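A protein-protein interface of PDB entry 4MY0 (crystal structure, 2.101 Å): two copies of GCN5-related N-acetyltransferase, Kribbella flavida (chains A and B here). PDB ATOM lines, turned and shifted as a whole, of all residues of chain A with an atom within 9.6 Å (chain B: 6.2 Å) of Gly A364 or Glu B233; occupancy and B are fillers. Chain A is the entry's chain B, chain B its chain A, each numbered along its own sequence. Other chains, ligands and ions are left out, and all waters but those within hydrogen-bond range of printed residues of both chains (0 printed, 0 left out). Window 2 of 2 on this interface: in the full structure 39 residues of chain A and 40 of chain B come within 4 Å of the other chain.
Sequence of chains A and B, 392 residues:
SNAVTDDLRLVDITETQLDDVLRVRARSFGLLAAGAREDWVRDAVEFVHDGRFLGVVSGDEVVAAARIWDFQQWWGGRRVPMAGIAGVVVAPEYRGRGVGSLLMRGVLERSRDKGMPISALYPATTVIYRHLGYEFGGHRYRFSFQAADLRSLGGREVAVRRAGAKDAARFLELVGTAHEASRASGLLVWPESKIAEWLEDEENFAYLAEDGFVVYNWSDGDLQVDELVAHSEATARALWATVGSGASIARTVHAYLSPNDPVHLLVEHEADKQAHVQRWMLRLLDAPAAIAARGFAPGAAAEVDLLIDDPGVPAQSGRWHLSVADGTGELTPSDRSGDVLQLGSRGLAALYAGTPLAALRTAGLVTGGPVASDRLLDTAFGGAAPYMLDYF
N of Glu B233 lies close to O of Thr A362 (3.4 Å).
OD1 of Asp B211 is in hydrogen-bond range of OG of Ser B232, at 2.8 Å.
The side-chain carboxylate (OE1) of Glu B233 is in salt-bridge range of the guanidinium group (NE) of Arg B237 (2.7 Å).
The backbone carbonyl oxygen (O) of Ala A358 lies within hydrogen-bond range of the side-chain hydroxyl (OG1) of Thr A362.
O of Asp B211 is in hydrogen-bond range of N of His B231, 3.0 Å away.
OG of Ser B232 is in hydrogen-bond range of OG1 of Thr B235, at 3.2 Å.
Thr A362 touches His B231 (OG1 to O, 3.7 Å).
Thr A362 touches Ser B232 (CG2 to O, 3.96 Å).
Glu B233 touches Ala A363 (CD to O, 3.8 Å).
Ala A363 touches Leu B266.
CA of Gly A364 touches OE2 of Glu B233 (3.6 Å).
Arg A346 touches none of the printed residues of chain B.
Of the printed residues of chain B, Thr A362 touches His B231, Ser B232 and Glu B233.
Gly A364 touches just one residue of chain B: Glu B233 (3.6 Å).
Of chain A, only Thr A362 (3.96 Å) comes within 4 Å of Ser B232.
Of the printed residues of chain A, Glu B233 touches Thr A362, Ala A363 and Gly A364.
Ala B234 touches none of the printed residues of chain A.
No residue of chain A comes within 4 Å of Ala B236.
Printed residues of chain A within 4 Å of Leu B266: Ala A363.
Of the 10 printed residues of chain B, 4 touch a printed residue of chain A.
Printed residues of chain B that touch a printed residue of chain A: His B231, Ser B232, Glu B233 and Leu B266.
Hydrophobic or aromatic side chains of chain B within 4 Å of the printed part of chain A: Leu B266.
Printed residues of chain A that touch a printed residue of chain B: Thr A362, Ala A363 and Gly A364.
Among the printed residues, 6 pairs touch across the chains.
Among the printed residues, no Asp or Glu carboxylate lies within 4 Å of a Lys or Arg side-chain nitrogen of the other chain.
No position is printed for both chains.
Of the 6 pairs that touch across the chains among the printed residues, none has its exchanged pair printed and touching as well.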
ATOM      1  N   GLU A 135     -16.909 -33.409 -24.470  1.00  0.00           N
ATOM      2  CA  GLU A 135     -17.654 -32.168 -24.685  1.00  0.00           C
ATOM      3  C   GLU A 135     -16.888 -31.299 -25.656  1.00  0.00           C
ATOM      4  O   GLU A 135     -15.677 -31.482 -25.802  1.00  0.00           O
ATOM      5  CB  GLU A 135     -17.910 -31.424 -23.360  1.00  0.00           C
ATOM      6  CG  GLU A 135     -18.905 -30.257 -23.496  1.00  0.00           C
ATOM      7  CD  GLU A 135     -20.159 -30.648 -24.293  1.00  0.00           C
ATOM      8  OE1 GLU A 135     -20.245 -30.310 -25.506  1.00  0.00           O
ATOM      9  OE2 GLU A 135     -21.061 -31.295 -23.708  1.00  0.00           O
ATOM     10  N   GLN A 342     -18.309 -28.419  -8.411  1.00  0.00           N
ATOM     11  CA  GLN A 342     -18.566 -29.814  -8.729  1.00  0.00           C
ATOM     12  C   GLN A 342     -18.728 -29.954 -10.236  1.00  0.00           C
ATOM     13  O   GLN A 342     -19.457 -29.175 -10.859  1.00  0.00           O
ATOM     14  CB  GLN A 342     -19.829 -30.277  -8.003  1.00  0.00           C
ATOM     15  CG  GLN A 342     -20.045 -31.768  -8.002  1.00  0.00           C
ATOM     16  CD  GLN A 342     -21.002 -32.193  -6.911  1.00  0.00           C
ATOM     17  OE1 GLN A 342     -21.446 -33.340  -6.869  1.00  0.00           O
ATOM     18  NE2 GLN A 342     -21.325 -31.266  -6.014  1.00  0.00           N
ATOM     19  N   LEU A 343     -18.054 -30.931 -10.834  1.00  0.00           N
ATOM     20  CA  LEU A 343     -18.150 -31.086 -12.283  1.00  0.00           C
ATOM     21  C   LEU A 343     -18.030 -32.531 -12.772  1.00  0.00           C
ATOM     22  O   LEU A 343     -17.316 -33.343 -12.189  1.00  0.00           O
ATOM     23  CB  LEU A 343     -17.173 -30.147 -13.009  1.00  0.00           C
ATOM     24  CG  LEU A 343     -15.665 -30.096 -12.758  1.00  0.00           C
ATOM     25  CD1 LEU A 343     -15.011 -29.128 -13.746  1.00  0.00           C
ATOM     26  CD2 LEU A 343     -15.311 -29.683 -11.347  1.00  0.00           C
ATOM     27  N   GLY A 344     -18.765 -32.848 -13.832  1.00  0.00           N
ATOM     28  CA  GLY A 344     -18.667 -34.155 -14.447  1.00  0.00           C
ATOM     29  C   GLY A 344     -17.566 -34.127 -15.493  1.00  0.00           C
ATOM     30  O   GLY A 344     -16.860 -33.124 -15.647  1.00  0.00           O
ATOM     31  N   SER A 345     -17.419 -35.229 -16.219  1.00  0.00           N
ATOM     32  CA  SER A 345     -16.419 -35.324 -17.267  1.00  0.00           C
ATOM     33  C   SER A 345     -16.586 -34.227 -18.330  1.00  0.00           C
ATOM     34  O   SER A 345     -15.589 -33.656 -18.796  1.00  0.00           O
ATOM     35  CB  SER A 345     -16.462 -36.712 -17.909  1.00  0.00           C
ATOM     36  OG  SER A 345     -15.611 -36.748 -19.042  1.00  0.00           O
ATOM     37  N   ARG A 346     -17.830 -33.931 -18.716  1.00  0.00           N
ATOM     38  CA  ARG A 346     -18.070 -32.910 -19.742  1.00  0.00           C
ATOM     39  C   ARG A 346     -17.604 -31.526 -19.298  1.00  0.00           C
ATOM     40  O   ARG A 346     -16.858 -30.849 -20.020  1.00  0.00           O
ATOM     41  CB  ARG A 346     -19.542 -32.870 -20.173  1.00  0.00           C
ATOM     42  CG  ARG A 346     -20.027 -34.155 -20.820  1.00  0.00           C
ATOM     43  CD  ARG A 346     -21.546 -34.162 -20.950  1.00  0.00           C
ATOM     44  NE  ARG A 346     -22.007 -33.031 -21.758  1.00  0.00           N
ATOM     45  CZ  ARG A 346     -23.275 -32.631 -21.825  1.00  0.00           C
ATOM     46  NH1 ARG A 346     -23.600 -31.600 -22.589  1.00  0.00           N
ATOM     47  NH2 ARG A 346     -24.219 -33.259 -21.122  1.00  0.00           N
ATOM     48  N   GLY A 347     -18.030 -31.117 -18.105  1.00  0.00           N
ATOM     49  CA  GLY A 347     -17.585 -29.853 -17.525  1.00  0.00           C
ATOM     50  C   GLY A 347     -16.075 -29.784 -17.318  1.00  0.00           C
ATOM     51  O   GLY A 347     -15.455 -28.741 -17.527  1.00  0.00           O
ATOM     52  N   LEU A 348     -15.478 -30.895 -16.894  1.00  0.00           N
ATOM     53  CA  LEU A 348     -14.036 -30.943 -16.675  1.00  0.00           C
ATOM     54  C   LEU A 348     -13.283 -30.692 -17.982  1.00  0.00           C
ATOM     55  O   LEU A 348     -12.362 -29.881 -18.021  1.00  0.00           O
ATOM     56  CB  LEU A 348     -13.619 -32.284 -16.054  1.00  0.00           C
ATOM     57  CG  LEU A 348     -12.132 -32.502 -15.770  1.00  0.00           C
ATOM     58  CD1 LEU A 348     -11.632 -31.545 -14.694  1.00  0.00           C
ATOM     59  CD2 LEU A 348     -11.878 -33.946 -15.349  1.00  0.00           C
ATOM     60  N   PRO A 356     -15.612 -20.614 -20.709  1.00  0.00           N
ATOM     61  CA  PRO A 356     -15.980 -19.740 -19.586  1.00  0.00           C
ATOM     62  C   PRO A 356     -16.907 -20.415 -18.567  1.00  0.00           C
ATOM     63  O   PRO A 356     -17.885 -21.066 -18.964  1.00  0.00           O
ATOM     64  CB  PRO A 356     -16.711 -18.581 -20.272  1.00  0.00           C
ATOM     65  CG  PRO A 356     -16.144 -18.548 -21.675  1.00  0.00           C
ATOM     66  CD  PRO A 356     -15.877 -19.988 -22.023  1.00  0.00           C
ATOM     67  N   LEU A 357     -16.600 -20.256 -17.279  1.00  0.00           N
ATOM     68  CA  LEU A 357     -17.412 -20.855 -16.222  1.00  0.00           C
ATOM     69  C   LEU A 357     -18.879 -20.440 -16.344  1.00  0.00           C
ATOM     70  O   LEU A 357     -19.779 -21.229 -16.048  1.00  0.00           O
ATOM     71  CB  LEU A 357     -16.883 -20.475 -14.835  1.00  0.00           C
ATOM     72  CG  LEU A 357     -15.922 -21.442 -14.145  1.00  0.00           C
ATOM     73  CD1 LEU A 357     -16.527 -22.824 -14.065  1.00  0.00           C
ATOM     74  CD2 LEU A 357     -14.619 -21.488 -14.896  1.00  0.00           C
ATOM     75  N   ALA A 358     -19.107 -19.198 -16.769  1.00  0.00           N
ATOM     76  CA  ALA A 358     -20.458 -18.665 -16.912  1.00  0.00           C
ATOM     77  C   ALA A 358     -21.266 -19.544 -17.855  1.00  0.00           C
ATOM     78  O   ALA A 358     -22.385 -19.940 -17.537  1.00  0.00           O
ATOM     79  CB  ALA A 358     -20.415 -17.234 -17.424  1.00  0.00           C
ATOM     80  N   ALA A 359     -20.680 -19.855 -19.008  1.00  0.00           N
ATOM     81  CA  ALA A 359     -21.310 -20.732 -19.990  1.00  0.00           C
ATOM     82  C   ALA A 359     -21.544 -22.134 -19.420  1.00  0.00           C
ATOM     83  O   ALA A 359     -22.576 -22.751 -19.676  1.00  0.00           O
ATOM     84  CB  ALA A 359     -20.446 -20.812 -21.269  1.00  0.00           C
ATOM     85  N   LEU A 360     -20.570 -22.643 -18.671  1.00  0.00           N
ATOM     86  CA  LEU A 360     -20.652 -23.999 -18.126  1.00  0.00           C
ATOM     87  C   LEU A 360     -21.714 -24.107 -17.056  1.00  0.00           C
ATOM     88  O   LEU A 360     -22.359 -25.158 -16.909  1.00  0.00           O
ATOM     89  CB  LEU A 360     -19.301 -24.447 -17.565  1.00  0.00           C
ATOM     90  CG  LEU A 360     -18.214 -24.539 -18.624  1.00  0.00           C
ATOM     91  CD1 LEU A 360     -16.895 -24.960 -18.021  1.00  0.00           C
ATOM     92  CD2 LEU A 360     -18.644 -25.496 -19.717  1.00  0.00           C
ATOM     93  N   ARG A 361     -21.909 -23.032 -16.299  1.00  0.00           N
ATOM     94  CA  ARG A 361     -22.966 -23.048 -15.292  1.00  0.00           C
ATOM     95  C   ARG A 361     -24.332 -23.027 -15.950  1.00  0.00           C
ATOM     96  O   ARG A 361     -25.227 -23.762 -15.547  1.00  0.00           O
ATOM     97  CB  ARG A 361     -22.833 -21.883 -14.315  1.00  0.00           C
ATOM     98  CG  ARG A 361     -21.661 -22.022 -13.385  1.00  0.00           C
ATOM     99  CD  ARG A 361     -21.716 -20.997 -12.279  1.00  0.00           C
ATOM    100  NE  ARG A 361     -20.568 -21.136 -11.394  1.00  0.00           N
ATOM    101  CZ  ARG A 361     -20.558 -21.905 -10.314  1.00  0.00           C
ATOM    102  NH1 ARG A 361     -19.472 -21.965  -9.553  1.00  0.00           N
ATOM    103  NH2 ARG A 361     -21.638 -22.602  -9.982  1.00  0.00           N
ATOM    104  N   THR A 362     -24.484 -22.191 -16.975  1.00  0.00           N
ATOM    105  CA  THR A 362     -25.754 -22.102 -17.686  1.00  0.00           C
ATOM    106  C   THR A 362     -26.093 -23.410 -18.414  1.00  0.00           C
ATOM    107  O   THR A 362     -27.245 -23.791 -18.493  1.00  0.00           O
ATOM    108  CB  THR A 362     -25.777 -20.883 -18.627  1.00  0.00           C
ATOM    109  OG1 THR A 362     -25.610 -19.694 -17.841  1.00  0.00           O
ATOM    110  CG2 THR A 362     -27.112 -20.799 -19.387  1.00  0.00           C
ATOM    111  N   ALA A 363     -25.083 -24.114 -18.911  1.00  0.00           N
ATOM    112  CA  ALA A 363     -25.306 -25.405 -19.567  1.00  0.00           C
ATOM    113  C   ALA A 363     -25.516 -26.523 -18.548  1.00  0.00           C
ATOM    114  O   ALA A 363     -25.820 -27.658 -18.914  1.00  0.00           O
ATOM    115  CB  ALA A 363     -24.127 -25.741 -20.481  1.00  0.00           C
ATOM    116  N   GLY A 364     -25.331 -26.213 -17.269  1.00  0.00           N
ATOM    117  CA  GLY A 364     -25.556 -27.193 -16.209  1.00  0.00           C
ATOM    118  C   GLY A 364     -24.436 -28.218 -16.074  1.00  0.00           C
ATOM    119  O   GLY A 364     -24.603 -29.240 -15.419  1.00  0.00           O
ATOM    120  N   LEU A 365     -23.285 -27.951 -16.677  1.00  0.00           N
ATOM    121  CA  LEU A 365     -22.179 -28.910 -16.633  1.00  0.00           C
ATOM    122  C   LEU A 365     -21.341 -28.778 -15.361  1.00  0.00           C
ATOM    123  O   LEU A 365     -20.517 -29.645 -15.033  1.00  0.00           O
ATOM    124  CB  LEU A 365     -21.283 -28.732 -17.850  1.00  0.00           C
ATOM    125  CG  LEU A 365     -21.649 -29.507 -19.124  1.00  0.00           C
ATOM    126  CD1 LEU A 365     -23.104 -29.952 -19.162  1.00  0.00           C
ATOM    127  CD2 LEU A 365     -21.272 -28.725 -20.371  1.00  0.00           C
ATOM    128  N   VAL A 366     -21.565 -27.681 -14.648  1.00  0.00           N
ATOM    129  CA  VAL A 366     -20.772 -27.312 -13.481  1.00  0.00           C
ATOM    130  C   VAL A 366     -21.741 -26.754 -12.439  1.00  0.00           C
ATOM    131  O   VAL A 366     -22.670 -26.021 -12.789  1.00  0.00           O
ATOM    132  CB  VAL A 366     -19.738 -26.238 -13.878  1.00  0.00           C
ATOM    133  CG1 VAL A 366     -19.376 -25.370 -12.706  1.00  0.00           C
ATOM    134  CG2 VAL A 366     -18.490 -26.884 -14.524  1.00  0.00           C
ATOM    135  N   THR A 367     -21.542 -27.098 -11.171  1.00  0.00           N
ATOM    136  CA  THR A 367     -22.471 -26.670 -10.128  1.00  0.00           C
ATOM    137  C   THR A 367     -21.779 -26.425  -8.778  1.00  0.00           C
ATOM    138  O   THR A 367     -20.685 -26.938  -8.538  1.00  0.00           O
ATOM    139  CB  THR A 367     -23.610 -27.707  -9.971  1.00  0.00           C
ATOM    140  OG1 THR A 367     -24.759 -27.088  -9.379  1.00  0.00           O
ATOM    141  CG2 THR A 367     -23.150 -28.881  -9.122  1.00  0.00           C
ATOM    142  N   GLY A 368     -22.411 -25.631  -7.911  1.00  0.00           N
ATOM    143  CA  GLY A 368     -21.851 -25.281  -6.608  1.00  0.00           C
ATOM    144  C   GLY A 368     -20.611 -24.400  -6.681  1.00  0.00           C
ATOM    145  O   GLY A 368     -20.197 -23.982  -7.762  1.00  0.00           O
ATOM    146  N   ASP B 211     -35.568 -15.256 -15.037  1.00  0.00           N
ATOM    147  CA  ASP B 211     -34.129 -14.995 -15.148  1.00  0.00           C
ATOM    148  C   ASP B 211     -33.608 -15.086 -16.576  1.00  0.00           C
ATOM    149  O   ASP B 211     -32.502 -15.579 -16.834  1.00  0.00           O
ATOM    150  CB  ASP B 211     -33.345 -15.938 -14.228  1.00  0.00           C
ATOM    151  CG  ASP B 211     -33.483 -17.386 -14.639  1.00  0.00           C
ATOM    152  OD1 ASP B 211     -32.547 -18.173 -14.380  1.00  0.00           O
ATOM    153  OD2 ASP B 211     -34.525 -17.732 -15.237  1.00  0.00           O
ATOM    154  N   HIS B 231     -29.882 -16.990 -17.313  1.00  0.00           N
ATOM    155  CA  HIS B 231     -28.979 -17.162 -16.183  1.00  0.00           C
ATOM    156  C   HIS B 231     -28.864 -18.610 -15.709  1.00  0.00           C
ATOM    157  O   HIS B 231     -27.887 -18.969 -15.053  1.00  0.00           O
ATOM    158  CB  HIS B 231     -29.432 -16.287 -15.009  1.00  0.00           C
ATOM    159  CG  HIS B 231     -29.408 -14.821 -15.309  1.00  0.00           C
ATOM    160  ND1 HIS B 231     -29.898 -13.874 -14.435  1.00  0.00           N
ATOM    161  CD2 HIS B 231     -28.956 -14.139 -16.389  1.00  0.00           C
ATOM    162  CE1 HIS B 231     -29.746 -12.671 -14.963  1.00  0.00           C
ATOM    163  NE2 HIS B 231     -29.175 -12.804 -16.147  1.00  0.00           N
ATOM    164  N   SER B 232     -29.858 -19.433 -16.030  1.00  0.00           N
ATOM    165  CA  SER B 232     -29.871 -20.823 -15.581  1.00  0.00           C
ATOM    166  C   SER B 232     -30.192 -21.770 -16.732  1.00  0.00           C
ATOM    167  O   SER B 232     -30.695 -21.345 -17.780  1.00  0.00           O
ATOM    168  CB  SER B 232     -30.880 -21.020 -14.439  1.00  0.00           C
ATOM    169  OG  SER B 232     -32.210 -20.887 -14.930  1.00  0.00           O
ATOM    170  N   GLU B 233     -29.901 -23.053 -16.528  1.00  0.00           N
ATOM    171  CA  GLU B 233     -30.088 -24.069 -17.558  1.00  0.00           C
ATOM    172  C   GLU B 233     -31.548 -24.246 -17.929  1.00  0.00           C
ATOM    173  O   GLU B 233     -31.895 -24.253 -19.114  1.00  0.00           O
ATOM    174  CB  GLU B 233     -29.531 -25.426 -17.092  1.00  0.00           C
ATOM    175  CG  GLU B 233     -29.599 -26.480 -18.206  1.00  0.00           C
ATOM    176  CD  GLU B 233     -29.432 -27.904 -17.706  1.00  0.00           C
ATOM    177  OE1 GLU B 233     -29.671 -28.841 -18.502  1.00  0.00           O
ATOM    178  OE2 GLU B 233     -29.063 -28.077 -16.526  1.00  0.00           O
ATOM    179  N   ALA B 234     -32.395 -24.414 -16.911  1.00  0.00           N
ATOM    180  CA  ALA B 234     -33.831 -24.577 -17.138  1.00  0.00           C
ATOM    181  C   ALA B 234     -34.398 -23.444 -18.002  1.00  0.00           C
ATOM    182  O   ALA B 234     -35.174 -23.678 -18.944  1.00  0.00           O
ATOM    183  CB  ALA B 234     -34.582 -24.696 -15.798  1.00  0.00           C
ATOM    184  N   THR B 235     -33.986 -22.219 -17.698  1.00  0.00           N
ATOM    185  CA  THR B 235     -34.481 -21.052 -18.423  1.00  0.00           C
ATOM    186  C   THR B 235     -33.933 -20.993 -19.843  1.00  0.00           C
ATOM    187  O   THR B 235     -34.656 -20.632 -20.782  1.00  0.00           O
ATOM    188  CB  THR B 235     -34.142 -19.768 -17.651  1.00  0.00           C
ATOM    189  OG1 THR B 235     -34.798 -19.821 -16.378  1.00  0.00           O
ATOM    190  CG2 THR B 235     -34.596 -18.515 -18.402  1.00  0.00           C
ATOM    191  N   ALA B 236     -32.651 -21.332 -20.006  1.00  0.00           N
ATOM    192  CA  ALA B 236     -32.050 -21.386 -21.345  1.00  0.00           C
ATOM    193  C   ALA B 236     -32.805 -22.404 -22.191  1.00  0.00           C
ATOM    194  O   ALA B 236     -33.145 -22.143 -23.344  1.00  0.00           O
ATOM    195  CB  ALA B 236     -30.558 -21.750 -21.267  1.00  0.00           C
ATOM    196  N   ARG B 237     -33.069 -23.566 -21.602  1.00  0.00           N
ATOM    197  CA  ARG B 237     -33.852 -24.577 -22.283  1.00  0.00           C
ATOM    198  C   ARG B 237     -35.241 -24.033 -22.664  1.00  0.00           C
ATOM    199  O   ARG B 237     -35.676 -24.189 -23.801  1.00  0.00           O
ATOM    200  CB  ARG B 237     -33.969 -25.828 -21.402  1.00  0.00           C
ATOM    201  CG  ARG B 237     -32.672 -26.622 -21.307  1.00  0.00           C
ATOM    202  CD  ARG B 237     -32.797 -27.861 -20.387  1.00  0.00           C
ATOM    203  NE  ARG B 237     -31.552 -28.630 -20.436  1.00  0.00           N
ATOM    204  CZ  ARG B 237     -31.280 -29.535 -21.377  1.00  0.00           C
ATOM    205  NH1 ARG B 237     -32.174 -29.797 -22.329  1.00  0.00           N
ATOM    206  NH2 ARG B 237     -30.128 -30.197 -21.360  1.00  0.00           N
ATOM    207  N   ALA B 238     -35.921 -23.378 -21.723  1.00  0.00           N
ATOM    208  CA  ALA B 238     -37.304 -22.919 -21.943  1.00  0.00           C
ATOM    209  C   ALA B 238     -37.360 -21.886 -23.047  1.00  0.00           C
ATOM    210  O   ALA B 238     -38.285 -21.873 -23.870  1.00  0.00           O
ATOM    211  CB  ALA B 238     -37.880 -22.306 -20.661  1.00  0.00           C
ATOM    212  N   LEU B 266     -25.793 -27.501 -25.194  1.00  0.00           N
ATOM    213  CA  LEU B 266     -27.101 -28.064 -24.882  1.00  0.00           C
ATOM    214  C   LEU B 266     -27.746 -28.817 -26.050  1.00  0.00           C
ATOM    215  O   LEU B 266     -28.296 -29.893 -25.861  1.00  0.00           O
ATOM    216  CB  LEU B 266     -28.041 -26.946 -24.429  1.00  0.00           C
ATOM    217  CG  LEU B 266     -27.738 -26.404 -23.032  1.00  0.00           C
ATOM    218  CD1 LEU B 266     -28.654 -25.239 -22.707  1.00  0.00           C
ATOM    219  CD2 LEU B 266     -27.883 -27.511 -22.001  1.00  0.00           C
